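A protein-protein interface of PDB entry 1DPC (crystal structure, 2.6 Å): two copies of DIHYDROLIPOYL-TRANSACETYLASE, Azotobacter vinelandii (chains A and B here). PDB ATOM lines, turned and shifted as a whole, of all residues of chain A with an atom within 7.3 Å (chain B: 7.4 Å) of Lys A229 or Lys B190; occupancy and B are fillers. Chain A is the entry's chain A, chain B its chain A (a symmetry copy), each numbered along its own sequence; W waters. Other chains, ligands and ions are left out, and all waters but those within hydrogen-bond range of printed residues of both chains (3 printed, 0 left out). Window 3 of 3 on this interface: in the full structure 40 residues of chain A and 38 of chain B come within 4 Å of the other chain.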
ATOM      1  N   GLN A  43       7.572 -26.169 -10.731  1.00  0.00           N
ATOM      2  CA  GLN A  43       8.396 -25.308 -11.547  1.00  0.00           C
ATOM      3  C   GLN A  43       7.511 -24.829 -12.689  1.00  0.00           C
ATOM      4  O   GLN A  43       6.928 -25.640 -13.399  1.00  0.00           O
ATOM      5  CB  GLN A  43       9.556 -26.090 -12.093  1.00  0.00           C
ATOM      6  CG  GLN A  43      10.303 -25.299 -13.142  1.00  0.00           C
ATOM      7  CD  GLN A  43      11.109 -24.128 -12.633  1.00  0.00           C
ATOM      8  OE1 GLN A  43      11.901 -24.277 -11.724  1.00  0.00           O
ATOM      9  NE2 GLN A  43      10.945 -22.960 -13.223  1.00  0.00           N
ATOM     10  N   GLU A  45       6.922 -22.665 -16.296  1.00  0.00           N
ATOM     11  CA  GLU A  45       7.541 -22.205 -17.538  1.00  0.00           C
ATOM     12  C   GLU A  45       6.465 -21.886 -18.581  1.00  0.00           C
ATOM     13  O   GLU A  45       5.312 -22.313 -18.441  1.00  0.00           O
ATOM     14  CB  GLU A  45       8.445 -23.265 -18.107  1.00  0.00           C
ATOM     15  CG  GLU A  45       9.242 -22.845 -19.340  1.00  0.00           C
ATOM     16  CD  GLU A  45      10.177 -21.659 -19.091  1.00  0.00           C
ATOM     17  OE1 GLU A  45       9.760 -20.492 -19.125  1.00  0.00           O
ATOM     18  OE2 GLU A  45      11.347 -21.912 -18.829  1.00  0.00           O
ATOM     19  N   SER A  46       6.763 -21.124 -19.630  1.00  0.00           N
ATOM     20  CA  SER A  46       5.836 -20.929 -20.737  1.00  0.00           C
ATOM     21  C   SER A  46       6.520 -21.355 -22.015  1.00  0.00           C
ATOM     22  O   SER A  46       7.710 -21.061 -22.193  1.00  0.00           O
ATOM     23  CB  SER A  46       5.460 -19.503 -20.881  1.00  0.00           C
ATOM     24  OG  SER A  46       4.548 -19.169 -19.853  1.00  0.00           O
ATOM     25  N   ALA A  47       5.834 -22.047 -22.903  1.00  0.00           N
ATOM     26  CA  ALA A  47       6.460 -22.523 -24.112  1.00  0.00           C
ATOM     27  C   ALA A  47       5.836 -21.788 -25.286  1.00  0.00           C
ATOM     28  O   ALA A  47       4.647 -21.454 -25.258  1.00  0.00           O
ATOM     29  CB  ALA A  47       6.204 -23.992 -24.240  1.00  0.00           C
ATOM     30  N   LEU A  83      12.076 -36.247 -24.036  1.00  0.00           N
ATOM     31  CA  LEU A  83      12.804 -35.752 -22.885  1.00  0.00           C
ATOM     32  C   LEU A  83      13.006 -36.769 -21.789  1.00  0.00           C
ATOM     33  O   LEU A  83      14.051 -36.773 -21.157  1.00  0.00           O
ATOM     34  CB  LEU A  83      12.105 -34.590 -22.269  1.00  0.00           C
ATOM     35  CG  LEU A  83      12.519 -33.251 -22.756  1.00  0.00           C
ATOM     36  CD1 LEU A  83      11.737 -32.213 -21.995  1.00  0.00           C
ATOM     37  CD2 LEU A  83      14.017 -33.083 -22.569  1.00  0.00           C
ATOM     38  N   LEU A 210       3.150 -24.168 -18.579  1.00  0.00           N
ATOM     39  CA  LEU A 210       3.510 -25.501 -18.133  1.00  0.00           C
ATOM     40  C   LEU A 210       3.770 -25.459 -16.636  1.00  0.00           C
ATOM     41  O   LEU A 210       4.427 -24.517 -16.174  1.00  0.00           O
ATOM     42  CB  LEU A 210       4.768 -25.927 -18.854  1.00  0.00           C
ATOM     43  CG  LEU A 210       4.734 -25.927 -20.390  1.00  0.00           C
ATOM     44  CD1 LEU A 210       6.134 -26.068 -20.931  1.00  0.00           C
ATOM     45  CD2 LEU A 210       3.842 -27.062 -20.888  1.00  0.00           C
ATOM     46  N   ALA A 223      17.635 -29.513 -12.073  1.00  0.00           N
ATOM     47  CA  ALA A 223      17.224 -30.542 -13.016  1.00  0.00           C
ATOM     48  C   ALA A 223      15.829 -30.249 -13.541  1.00  0.00           C
ATOM     49  O   ALA A 223      15.558 -30.310 -14.744  1.00  0.00           O
ATOM     50  CB  ALA A 223      17.197 -31.881 -12.342  1.00  0.00           C
ATOM     51  N   ALA A 224      14.927 -29.859 -12.647  1.00  0.00           N
ATOM     52  CA  ALA A 224      13.577 -29.537 -13.066  1.00  0.00           C
ATOM     53  C   ALA A 224      13.518 -28.309 -13.959  1.00  0.00           C
ATOM     54  O   ALA A 224      12.804 -28.347 -14.961  1.00  0.00           O
ATOM     55  CB  ALA A 224      12.768 -29.280 -11.874  1.00  0.00           C
ATOM     56  N   ALA A 225      14.271 -27.233 -13.654  1.00  0.00           N
ATOM     57  CA  ALA A 225      14.321 -26.033 -14.492  1.00  0.00           C
ATOM     58  C   ALA A 225      14.858 -26.354 -15.870  1.00  0.00           C
ATOM     59  O   ALA A 225      14.400 -25.825 -16.873  1.00  0.00           O
ATOM     60  CB  ALA A 225      15.224 -24.965 -13.917  1.00  0.00           C
ATOM     61  N   ARG A 226      15.851 -27.234 -15.919  1.00  0.00           N
ATOM     62  CA  ARG A 226      16.411 -27.738 -17.153  1.00  0.00           C
ATOM     63  C   ARG A 226      15.348 -28.552 -17.871  1.00  0.00           C
ATOM     64  O   ARG A 226      15.246 -28.453 -19.092  1.00  0.00           O
ATOM     65  CB  ARG A 226      17.579 -28.573 -16.771  1.00  0.00           C
ATOM     66  CG  ARG A 226      18.643 -28.884 -17.789  1.00  0.00           C
ATOM     67  CD  ARG A 226      19.887 -29.343 -16.963  1.00  0.00           C
ATOM     68  NE  ARG A 226      20.436 -28.345 -16.041  1.00  0.00           N
ATOM     69  CZ  ARG A 226      21.177 -27.278 -16.414  1.00  0.00           C
ATOM     70  NH1 ARG A 226      21.509 -27.004 -17.684  1.00  0.00           N
ATOM     71  NH2 ARG A 226      21.544 -26.393 -15.483  1.00  0.00           N
ATOM     72  N   PHE A 227      14.507 -29.354 -17.222  1.00  0.00           N
ATOM     73  CA  PHE A 227      13.501 -30.107 -17.923  1.00  0.00           C
ATOM     74  C   PHE A 227      12.455 -29.187 -18.531  1.00  0.00           C
ATOM     75  O   PHE A 227      12.137 -29.372 -19.714  1.00  0.00           O
ATOM     76  CB  PHE A 227      12.817 -31.074 -16.983  1.00  0.00           C
ATOM     77  CG  PHE A 227      11.777 -32.014 -17.598  1.00  0.00           C
ATOM     78  CD1 PHE A 227      10.471 -31.575 -17.830  1.00  0.00           C
ATOM     79  CD2 PHE A 227      12.134 -33.328 -17.874  1.00  0.00           C
ATOM     80  CE1 PHE A 227       9.526 -32.451 -18.331  1.00  0.00           C
ATOM     81  CE2 PHE A 227      11.182 -34.202 -18.374  1.00  0.00           C
ATOM     82  CZ  PHE A 227       9.885 -33.762 -18.598  1.00  0.00           C
ATOM     83  N   THR A 228      11.870 -28.225 -17.815  1.00  0.00           N
ATOM     84  CA  THR A 228      10.841 -27.419 -18.449  1.00  0.00           C
ATOM     85  C   THR A 228      11.453 -26.542 -19.534  1.00  0.00           C
ATOM     86  O   THR A 228      10.810 -26.290 -20.555  1.00  0.00           O
ATOM     87  CB  THR A 228      10.092 -26.551 -17.397  1.00  0.00           C
ATOM     88  OG1 THR A 228      11.054 -26.006 -16.527  1.00  0.00           O
ATOM     89  CG2 THR A 228       9.100 -27.331 -16.587  1.00  0.00           C
ATOM     90  N   LYS A 229      12.711 -26.116 -19.405  1.00  0.00           N
ATOM     91  CA  LYS A 229      13.374 -25.332 -20.441  1.00  0.00           C
ATOM     92  C   LYS A 229      13.488 -26.146 -21.723  1.00  0.00           C
ATOM     93  O   LYS A 229      12.985 -25.694 -22.755  1.00  0.00           O
ATOM     94  CB  LYS A 229      14.775 -24.932 -20.002  1.00  0.00           C
ATOM     95  CG  LYS A 229      15.326 -23.829 -20.895  1.00  0.00           C
ATOM     96  CD  LYS A 229      16.707 -24.165 -21.422  1.00  0.00           C
ATOM     97  CE  LYS A 229      17.205 -22.980 -22.231  1.00  0.00           C
ATOM     98  NZ  LYS A 229      17.413 -21.821 -21.367  1.00  0.00           N
ATOM     99  N   ARG A 230      14.074 -27.360 -21.677  1.00  0.00           N
ATOM    100  CA  ARG A 230      14.183 -28.241 -22.822  1.00  0.00           C
ATOM    101  C   ARG A 230      12.826 -28.451 -23.409  1.00  0.00           C
ATOM    102  O   ARG A 230      12.700 -28.315 -24.620  1.00  0.00           O
ATOM    103  CB  ARG A 230      14.702 -29.614 -22.475  1.00  0.00           C
ATOM    104  CG  ARG A 230      16.168 -29.695 -22.167  1.00  0.00           C
ATOM    105  CD  ARG A 230      16.833 -29.414 -23.482  1.00  0.00           C
ATOM    106  NE  ARG A 230      16.765 -30.523 -24.421  1.00  0.00           N
ATOM    107  CZ  ARG A 230      16.577 -30.348 -25.735  1.00  0.00           C
ATOM    108  NH1 ARG A 230      16.408 -29.143 -26.288  1.00  0.00           N
ATOM    109  NH2 ARG A 230      16.709 -31.398 -26.537  1.00  0.00           N
ATOM    110  N   LEU A 231      11.804 -28.710 -22.590  1.00  0.00           N
ATOM    111  CA  LEU A 231      10.460 -28.897 -23.121  1.00  0.00           C
ATOM    112  C   LEU A 231       9.958 -27.633 -23.810  1.00  0.00           C
ATOM    113  O   LEU A 231       9.322 -27.724 -24.860  1.00  0.00           O
ATOM    114  CB  LEU A 231       9.497 -29.298 -21.993  1.00  0.00           C
ATOM    115  CG  LEU A 231       8.061 -29.650 -22.342  1.00  0.00           C
ATOM    116  CD1 LEU A 231       8.050 -30.802 -23.324  1.00  0.00           C
ATOM    117  CD2 LEU A 231       7.296 -30.001 -21.075  1.00  0.00           C
ATOM    118  N   GLY A 232      10.257 -26.449 -23.307  1.00  0.00           N
ATOM    119  CA  GLY A 232       9.830 -25.227 -23.948  1.00  0.00           C
ATOM    120  C   GLY A 232      10.500 -25.119 -25.309  1.00  0.00           C
ATOM    121  O   GLY A 232       9.886 -24.720 -26.298  1.00  0.00           O
ATOM    122  N   ASP A 233      11.767 -25.529 -25.354  1.00  0.00           N
ATOM    123  CA  ASP A 233      12.561 -25.579 -26.577  1.00  0.00           C
ATOM    124  C   ASP A 233      12.049 -26.577 -27.605  1.00  0.00           C
ATOM    125  O   ASP A 233      12.045 -26.287 -28.802  1.00  0.00           O
ATOM    126  CB  ASP A 233      14.000 -25.976 -26.320  1.00  0.00           C
ATOM    127  CG  ASP A 233      14.884 -24.969 -25.610  1.00  0.00           C
ATOM    128  OD1 ASP A 233      14.527 -23.782 -25.528  1.00  0.00           O
ATOM    129  OD2 ASP A 233      15.953 -25.401 -25.157  1.00  0.00           O
ATOM    130  N   LEU A 234      11.631 -27.763 -27.153  1.00  0.00           N
ATOM    131  CA  LEU A 234      11.115 -28.775 -28.030  1.00  0.00           C
ATOM    132  C   LEU A 234       9.782 -28.353 -28.552  1.00  0.00           C
ATOM    133  O   LEU A 234       9.532 -28.599 -29.710  1.00  0.00           O
ATOM    134  CB  LEU A 234      10.930 -30.110 -27.331  1.00  0.00           C
ATOM    135  CG  LEU A 234      12.185 -30.896 -27.000  1.00  0.00           C
ATOM    136  CD1 LEU A 234      11.761 -32.171 -26.318  1.00  0.00           C
ATOM    137  CD2 LEU A 234      12.960 -31.263 -28.250  1.00  0.00           C
ATOM    138  N   LEU A 235       8.899 -27.726 -27.795  1.00  0.00           N
ATOM    139  CA  LEU A 235       7.587 -27.335 -28.310  1.00  0.00           C
ATOM    140  C   LEU A 235       7.647 -26.116 -29.234  1.00  0.00           C
ATOM    141  O   LEU A 235       6.789 -25.888 -30.096  1.00  0.00           O
ATOM    142  CB  LEU A 235       6.649 -27.055 -27.126  1.00  0.00           C
ATOM    143  CG  LEU A 235       6.300 -28.177 -26.165  1.00  0.00           C
ATOM    144  CD1 LEU A 235       5.328 -27.626 -25.143  1.00  0.00           C
ATOM    145  CD2 LEU A 235       5.663 -29.353 -26.898  1.00  0.00           C
ATOM    146  N   SER B 165      18.855 -19.706  -6.502  1.00  0.00           N
ATOM    147  CA  SER B 165      18.705 -19.031  -7.777  1.00  0.00           C
ATOM    148  C   SER B 165      18.789 -19.986  -8.933  1.00  0.00           C
ATOM    149  O   SER B 165      19.815 -20.640  -9.143  1.00  0.00           O
ATOM    150  CB  SER B 165      19.775 -17.947  -7.909  1.00  0.00           C
ATOM    151  OG  SER B 165      19.771 -17.293  -9.180  1.00  0.00           O
ATOM    152  N   LEU B 166      17.717 -20.081  -9.721  1.00  0.00           N
ATOM    153  CA  LEU B 166      17.722 -20.927 -10.901  1.00  0.00           C
ATOM    154  C   LEU B 166      17.699 -20.054 -12.122  1.00  0.00           C
ATOM    155  O   LEU B 166      17.720 -20.597 -13.228  1.00  0.00           O
ATOM    156  CB  LEU B 166      16.512 -21.863 -10.911  1.00  0.00           C
ATOM    157  CG  LEU B 166      16.408 -22.792  -9.693  1.00  0.00           C
ATOM    158  CD1 LEU B 166      15.191 -23.665  -9.783  1.00  0.00           C
ATOM    159  CD2 LEU B 166      17.623 -23.669  -9.640  1.00  0.00           C
ATOM    160  N   GLY B 167      17.802 -18.728 -11.964  1.00  0.00           N
ATOM    161  CA  GLY B 167      17.731 -17.781 -13.075  1.00  0.00           C
ATOM    162  C   GLY B 167      18.626 -18.097 -14.272  1.00  0.00           C
ATOM    163  O   GLY B 167      18.329 -17.839 -15.436  1.00  0.00           O
ATOM    164  N   HIS B 168      19.747 -18.716 -13.985  1.00  0.00           N
ATOM    165  CA  HIS B 168      20.682 -19.137 -15.011  1.00  0.00           C
ATOM    166  C   HIS B 168      20.230 -20.313 -15.868  1.00  0.00           C
ATOM    167  O   HIS B 168      20.923 -20.642 -16.828  1.00  0.00           O
ATOM    168  CB  HIS B 168      22.022 -19.484 -14.354  1.00  0.00           C
ATOM    169  CG  HIS B 168      21.953 -20.490 -13.216  1.00  0.00           C
ATOM    170  ND1 HIS B 168      22.251 -21.788 -13.226  1.00  0.00           N
ATOM    171  CD2 HIS B 168      21.524 -20.169 -11.949  1.00  0.00           C
ATOM    172  CE1 HIS B 168      22.016 -22.268 -12.027  1.00  0.00           C
ATOM    173  NE2 HIS B 168      21.579 -21.285 -11.272  1.00  0.00           N
ATOM    174  N   ILE B 169      19.143 -21.014 -15.536  1.00  0.00           N
ATOM    175  CA  ILE B 169      18.750 -22.172 -16.310  1.00  0.00           C
ATOM    176  C   ILE B 169      17.479 -21.767 -16.987  1.00  0.00           C
ATOM    177  O   ILE B 169      17.415 -21.824 -18.214  1.00  0.00           O
ATOM    178  CB  ILE B 169      18.513 -23.372 -15.430  1.00  0.00           C
ATOM    179  CG1 ILE B 169      19.792 -23.662 -14.722  1.00  0.00           C
ATOM    180  CG2 ILE B 169      18.120 -24.586 -16.245  1.00  0.00           C
ATOM    181  CD1 ILE B 169      19.555 -24.597 -13.555  1.00  0.00           C
ATOM    182  N   GLY B 170      16.476 -21.350 -16.236  1.00  0.00           N
ATOM    183  CA  GLY B 170      15.298 -20.853 -16.896  1.00  0.00           C
ATOM    184  C   GLY B 170      14.125 -20.956 -15.979  1.00  0.00           C
ATOM    185  O   GLY B 170      14.282 -21.246 -14.795  1.00  0.00           O
ATOM    186  N   GLY B 171      12.945 -20.725 -16.506  1.00  0.00           N
ATOM    187  CA  GLY B 171      11.780 -20.816 -15.671  1.00  0.00           C
ATOM    188  C   GLY B 171      11.274 -19.452 -15.291  1.00  0.00           C
ATOM    189  O   GLY B 171      11.980 -18.452 -15.181  1.00  0.00           O
ATOM    190  N   THR B 172       9.987 -19.547 -15.054  1.00  0.00           N
ATOM    191  CA  THR B 172       9.155 -18.442 -14.663  1.00  0.00           C
ATOM    192  C   THR B 172       8.990 -18.242 -13.157  1.00  0.00           C
ATOM    193  O   THR B 172       8.814 -17.114 -12.692  1.00  0.00           O
ATOM    194  CB  THR B 172       7.882 -18.764 -15.411  1.00  0.00           C
ATOM    195  OG1 THR B 172       8.138 -18.145 -16.662  1.00  0.00           O
ATOM    196  CG2 THR B 172       6.598 -18.337 -14.786  1.00  0.00           C
ATOM    197  N   ALA B 173       9.070 -19.284 -12.339  1.00  0.00           N
ATOM    198  CA  ALA B 173       8.806 -19.213 -10.909  1.00  0.00           C
ATOM    199  C   ALA B 173       8.803 -20.672 -10.468  1.00  0.00           C
ATOM    200  O   ALA B 173       8.728 -21.574 -11.319  1.00  0.00           O
ATOM    201  CB  ALA B 173       7.415 -18.652 -10.601  1.00  0.00           C
ATOM    202  N   VAL B 188      14.669 -17.487  -7.008  1.00  0.00           N
ATOM    203  CA  VAL B 188      14.822 -16.464  -8.032  1.00  0.00           C
ATOM    204  C   VAL B 188      14.853 -17.176  -9.371  1.00  0.00           C
ATOM    205  O   VAL B 188      15.625 -18.138  -9.517  1.00  0.00           O
ATOM    206  CB  VAL B 188      16.135 -15.698  -7.852  1.00  0.00           C
ATOM    207  CG1 VAL B 188      16.212 -14.589  -8.879  1.00  0.00           C
ATOM    208  CG2 VAL B 188      16.202 -15.094  -6.460  1.00  0.00           C
ATOM    209  N   SER B 189      14.091 -16.738 -10.369  1.00  0.00           N
ATOM    210  CA  SER B 189      14.075 -17.412 -11.650  1.00  0.00           C
ATOM    211  C   SER B 189      14.575 -16.501 -12.764  1.00  0.00           C
ATOM    212  O   SER B 189      15.126 -15.455 -12.457  1.00  0.00           O
ATOM    213  CB  SER B 189      12.651 -17.892 -11.936  1.00  0.00           C
ATOM    214  OG  SER B 189      12.145 -18.882 -11.064  1.00  0.00           O
ATOM    215  N   LYS B 190      14.352 -16.821 -14.036  1.00  0.00           N
ATOM    216  CA  LYS B 190      14.966 -16.125 -15.130  1.00  0.00           C
ATOM    217  C   LYS B 190      14.284 -14.800 -15.357  1.00  0.00           C
ATOM    218  O   LYS B 190      13.053 -14.711 -15.283  1.00  0.00           O
ATOM    219  CB  LYS B 190      14.868 -16.997 -16.364  1.00  0.00           C
ATOM    220  CG  LYS B 190      15.913 -16.672 -17.393  1.00  0.00           C
ATOM    221  CD  LYS B 190      15.459 -17.045 -18.795  1.00  0.00           C
ATOM    222  CE  LYS B 190      16.657 -17.164 -19.748  1.00  0.00           C
ATOM    223  NZ  LYS B 190      17.404 -18.406 -19.551  1.00  0.00           N
ATOM    224  N   ALA B 191      15.111 -13.793 -15.641  1.00  0.00           N
ATOM    225  CA  ALA B 191      14.660 -12.440 -15.906  1.00  0.00           C
ATOM    226  C   ALA B 191      14.280 -12.300 -17.368  1.00  0.00           C
ATOM    227  O   ALA B 191      14.969 -12.815 -18.259  1.00  0.00           O
ATOM    228  CB  ALA B 191      15.765 -11.462 -15.583  1.00  0.00           C
ATOM    229  N   SER B 192      13.186 -11.585 -17.625  1.00  0.00           N
ATOM    230  CA  SER B 192      12.672 -11.398 -18.960  1.00  0.00           C
ATOM    231  C   SER B 192      12.323  -9.943 -19.120  1.00  0.00           C
ATOM    232  O   SER B 192      12.048  -9.230 -18.153  1.00  0.00           O
ATOM    233  CB  SER B 192      11.371 -12.144 -19.237  1.00  0.00           C
ATOM    234  OG  SER B 192      11.204 -13.329 -18.493  1.00  0.00           O
ATOM    235  N   MET B 193      12.302  -9.520 -20.373  1.00  0.00           N
ATOM    236  CA  MET B 193      11.855  -8.194 -20.725  1.00  0.00           C
ATOM    237  C   MET B 193      10.340  -8.274 -20.716  1.00  0.00           C
ATOM    238  O   MET B 193       9.759  -9.166 -21.326  1.00  0.00           O
ATOM    239  CB  MET B 193      12.342  -7.871 -22.088  1.00  0.00           C
ATOM    240  CG  MET B 193      12.559  -6.411 -22.249  1.00  0.00           C
ATOM    241  SD  MET B 193      14.146  -6.003 -21.507  1.00  0.00           S
ATOM    242  CE  MET B 193      13.548  -4.430 -21.029  1.00  0.00           C
ATOM    243  N   GLN B 194       9.680  -7.390 -20.012  1.00  0.00           N
ATOM    244  CA  GLN B 194       8.254  -7.449 -19.908  1.00  0.00           C
ATOM    245  C   GLN B 194       7.740  -6.064 -20.149  1.00  0.00           C
ATOM    246  O   GLN B 194       8.459  -5.109 -19.899  1.00  0.00           O
ATOM    247  CB  GLN B 194       7.823  -7.869 -18.532  1.00  0.00           C
ATOM    248  CG  GLN B 194       8.059  -9.322 -18.162  1.00  0.00           C
ATOM    249  CD  GLN B 194       7.468 -10.334 -19.125  1.00  0.00           C
ATOM    250  OE1 GLN B 194       6.428 -10.125 -19.757  1.00  0.00           O
ATOM    251  NE2 GLN B 194       8.118 -11.482 -19.228  1.00  0.00           N
ATOM    252  N   LEU B 206      13.089  -4.945 -17.463  1.00  0.00           N
ATOM    253  CA  LEU B 206      13.652  -6.256 -17.220  1.00  0.00           C
ATOM    254  C   LEU B 206      13.151  -6.630 -15.854  1.00  0.00           C
ATOM    255  O   LEU B 206      13.483  -5.971 -14.863  1.00  0.00           O
ATOM    256  CB  LEU B 206      15.167  -6.189 -17.218  1.00  0.00           C
ATOM    257  CG  LEU B 206      15.892  -7.498 -17.047  1.00  0.00           C
ATOM    258  CD1 LEU B 206      15.693  -8.331 -18.277  1.00  0.00           C
ATOM    259  CD2 LEU B 206      17.365  -7.262 -16.855  1.00  0.00           C
ATOM    260  N   MET B 207      12.342  -7.676 -15.844  1.00  0.00           N
ATOM    261  CA  MET B 207      11.667  -8.129 -14.650  1.00  0.00           C
ATOM    262  C   MET B 207      12.286  -9.404 -14.116  1.00  0.00           C
ATOM    263  O   MET B 207      12.512 -10.313 -14.910  1.00  0.00           O
ATOM    264  CB  MET B 207      10.231  -8.383 -14.983  1.00  0.00           C
ATOM    265  CG  MET B 207       9.537  -7.117 -15.424  1.00  0.00           C
ATOM    266  SD  MET B 207       9.138  -6.075 -14.012  1.00  0.00           S
ATOM    267  CE  MET B 207      10.018  -4.728 -14.632  1.00  0.00           C
ATOM    268  N   LEU B 208      12.583  -9.522 -12.819  1.00  0.00           N
ATOM    269  CA  LEU B 208      13.142 -10.727 -12.209  1.00  0.00           C
ATOM    270  C   LEU B 208      12.053 -11.392 -11.392  1.00  0.00           C
ATOM    271  O   LEU B 208      11.473 -10.719 -10.538  1.00  0.00           O
ATOM    272  CB  LEU B 208      14.289 -10.345 -11.294  1.00  0.00           C
ATOM    273  CG  LEU B 208      15.002 -11.403 -10.490  1.00  0.00           C
ATOM    274  CD1 LEU B 208      15.709 -12.324 -11.449  1.00  0.00           C
ATOM    275  CD2 LEU B 208      15.975 -10.759  -9.515  1.00  0.00           C
ATOM    276  N   PRO B 209      11.678 -12.655 -11.572  1.00  0.00           N
ATOM    277  CA  PRO B 209      10.613 -13.296 -10.817  1.00  0.00           C
ATOM    278  C   PRO B 209      11.169 -13.770  -9.488  1.00  0.00           C
ATOM    279  O   PRO B 209      12.223 -14.403  -9.432  1.00  0.00           O
ATOM    280  CB  PRO B 209      10.148 -14.415 -11.707  1.00  0.00           C
ATOM    281  CG  PRO B 209      10.839 -14.190 -13.029  1.00  0.00           C
ATOM    282  CD  PRO B 209      12.131 -13.526 -12.636  1.00  0.00           C
HETATM  283  O   HOH W   1       4.995 -19.188 -17.138  1.00  0.00           O
HETATM  284  O   HOH W   2      12.961 -21.110 -12.193  1.00  0.00           O
HETATM  285  O   HOH W   3      13.493 -20.259 -19.485  1.00  0.00           O
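Water W2 lies within hydrogen-bond range of the side-chain hydroxyl (OG) of Ser B189 (2.6 Å), the backbone carbonyl oxygen (O) of Gly B170 (2.9 Å) and the side-chain amide nitrogen (NE2) of Gln A43 (2.9 Å).
Water W1 lies within hydrogen-bond range of OG of Ser A46, OG1 of Thr B172 and O of Glu A45.
Water W3 lies within hydrogen-bond range of the side-chain carboxylate of Glu A45 and the backbone NH of Gly B171.
Of the 19 printed residues of chain A, 5 touch a printed residue of chain B.
Printed residues of chain A that touch a printed residue of chain B: Gln A43, Glu A45, Ala A225, Arg A226 and Lys A229.
Of the 20 printed residues of chain B, 7 touch a printed residue of chain A.
No position is printed for both chains.
Of the 11 pairs that touch across the chains among the printed residues, none has its exchanged pair printed and touching as well.
Printed residues of chain B within 4 Å of Arg A226: Ile B169 (3.3 Å).
Lys A229 touches just these residues of chain B: Ile B169 (3.2 Å) and Lys B190 (3.9 Å).
Gly B167 touches none of the printed residues of chain A.
Printed residues of chain A within 4 Å of Gly B170: Ala A225 (3.9 Å).
Lys B190 touches just one residue of chain A: Lys A229.
The nearest residue of chain B that does not touch Lys A229 is Gly B170 (5.0 Å).
The nearest printed residue of chain A that does not touch Leu B166 is Ala A225 (4.3 Å).
Among the printed residues, merely in contact across the chains: Gln A43 with Leu B166 (3.9 Å), Gln A43 with Gly B171 (3.4 Å), Gln A43 with Thr B172 (3.99 Å), Glu A45 with Thr B172 (3.8 Å), Ala A225 with Ile B169 (3.7 Å), Ala A225 with Gly B170 (3.9 Å), Arg A226 with Ile B169 (3.3 Å) and Lys A229 with Lys B190 (3.9 Å).
NZ of Lys A229 is in hydrogen-bond range of O of Ile B169.
The side-chain amide nitrogen (NE2) of Gln A43 is in hydrogen-bond range of the backbone carbonyl oxygen (O) of Ala B173 (3.2 Å).
OE2 of Glu A45 lies within hydrogen-bond range of N of Gly B171, at 3.1 Å.
O of Ala A225 lies within hydrogen-bond range of OG1 of Thr A228, 3.4 Å away.
The backbone NH (N) of Ala B173 lies within hydrogen-bond range of the side-chain hydroxyl (OG) of Ser B189 (3.4 Å).
The backbone NH (N) of Lys B190 lies within hydrogen-bond range of the backbone carbonyl oxygen (O) of Gly B171.
The backbone carbonyl oxygen of Glu A45 sits at hydrogen-bond distance from the backbone NH of Leu A210, 2.9 Å away.
The backbone NH (N) of Leu B166 is in hydrogen-bond range of the backbone carbonyl oxygen (O) of Val B188 (2.9 Å).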
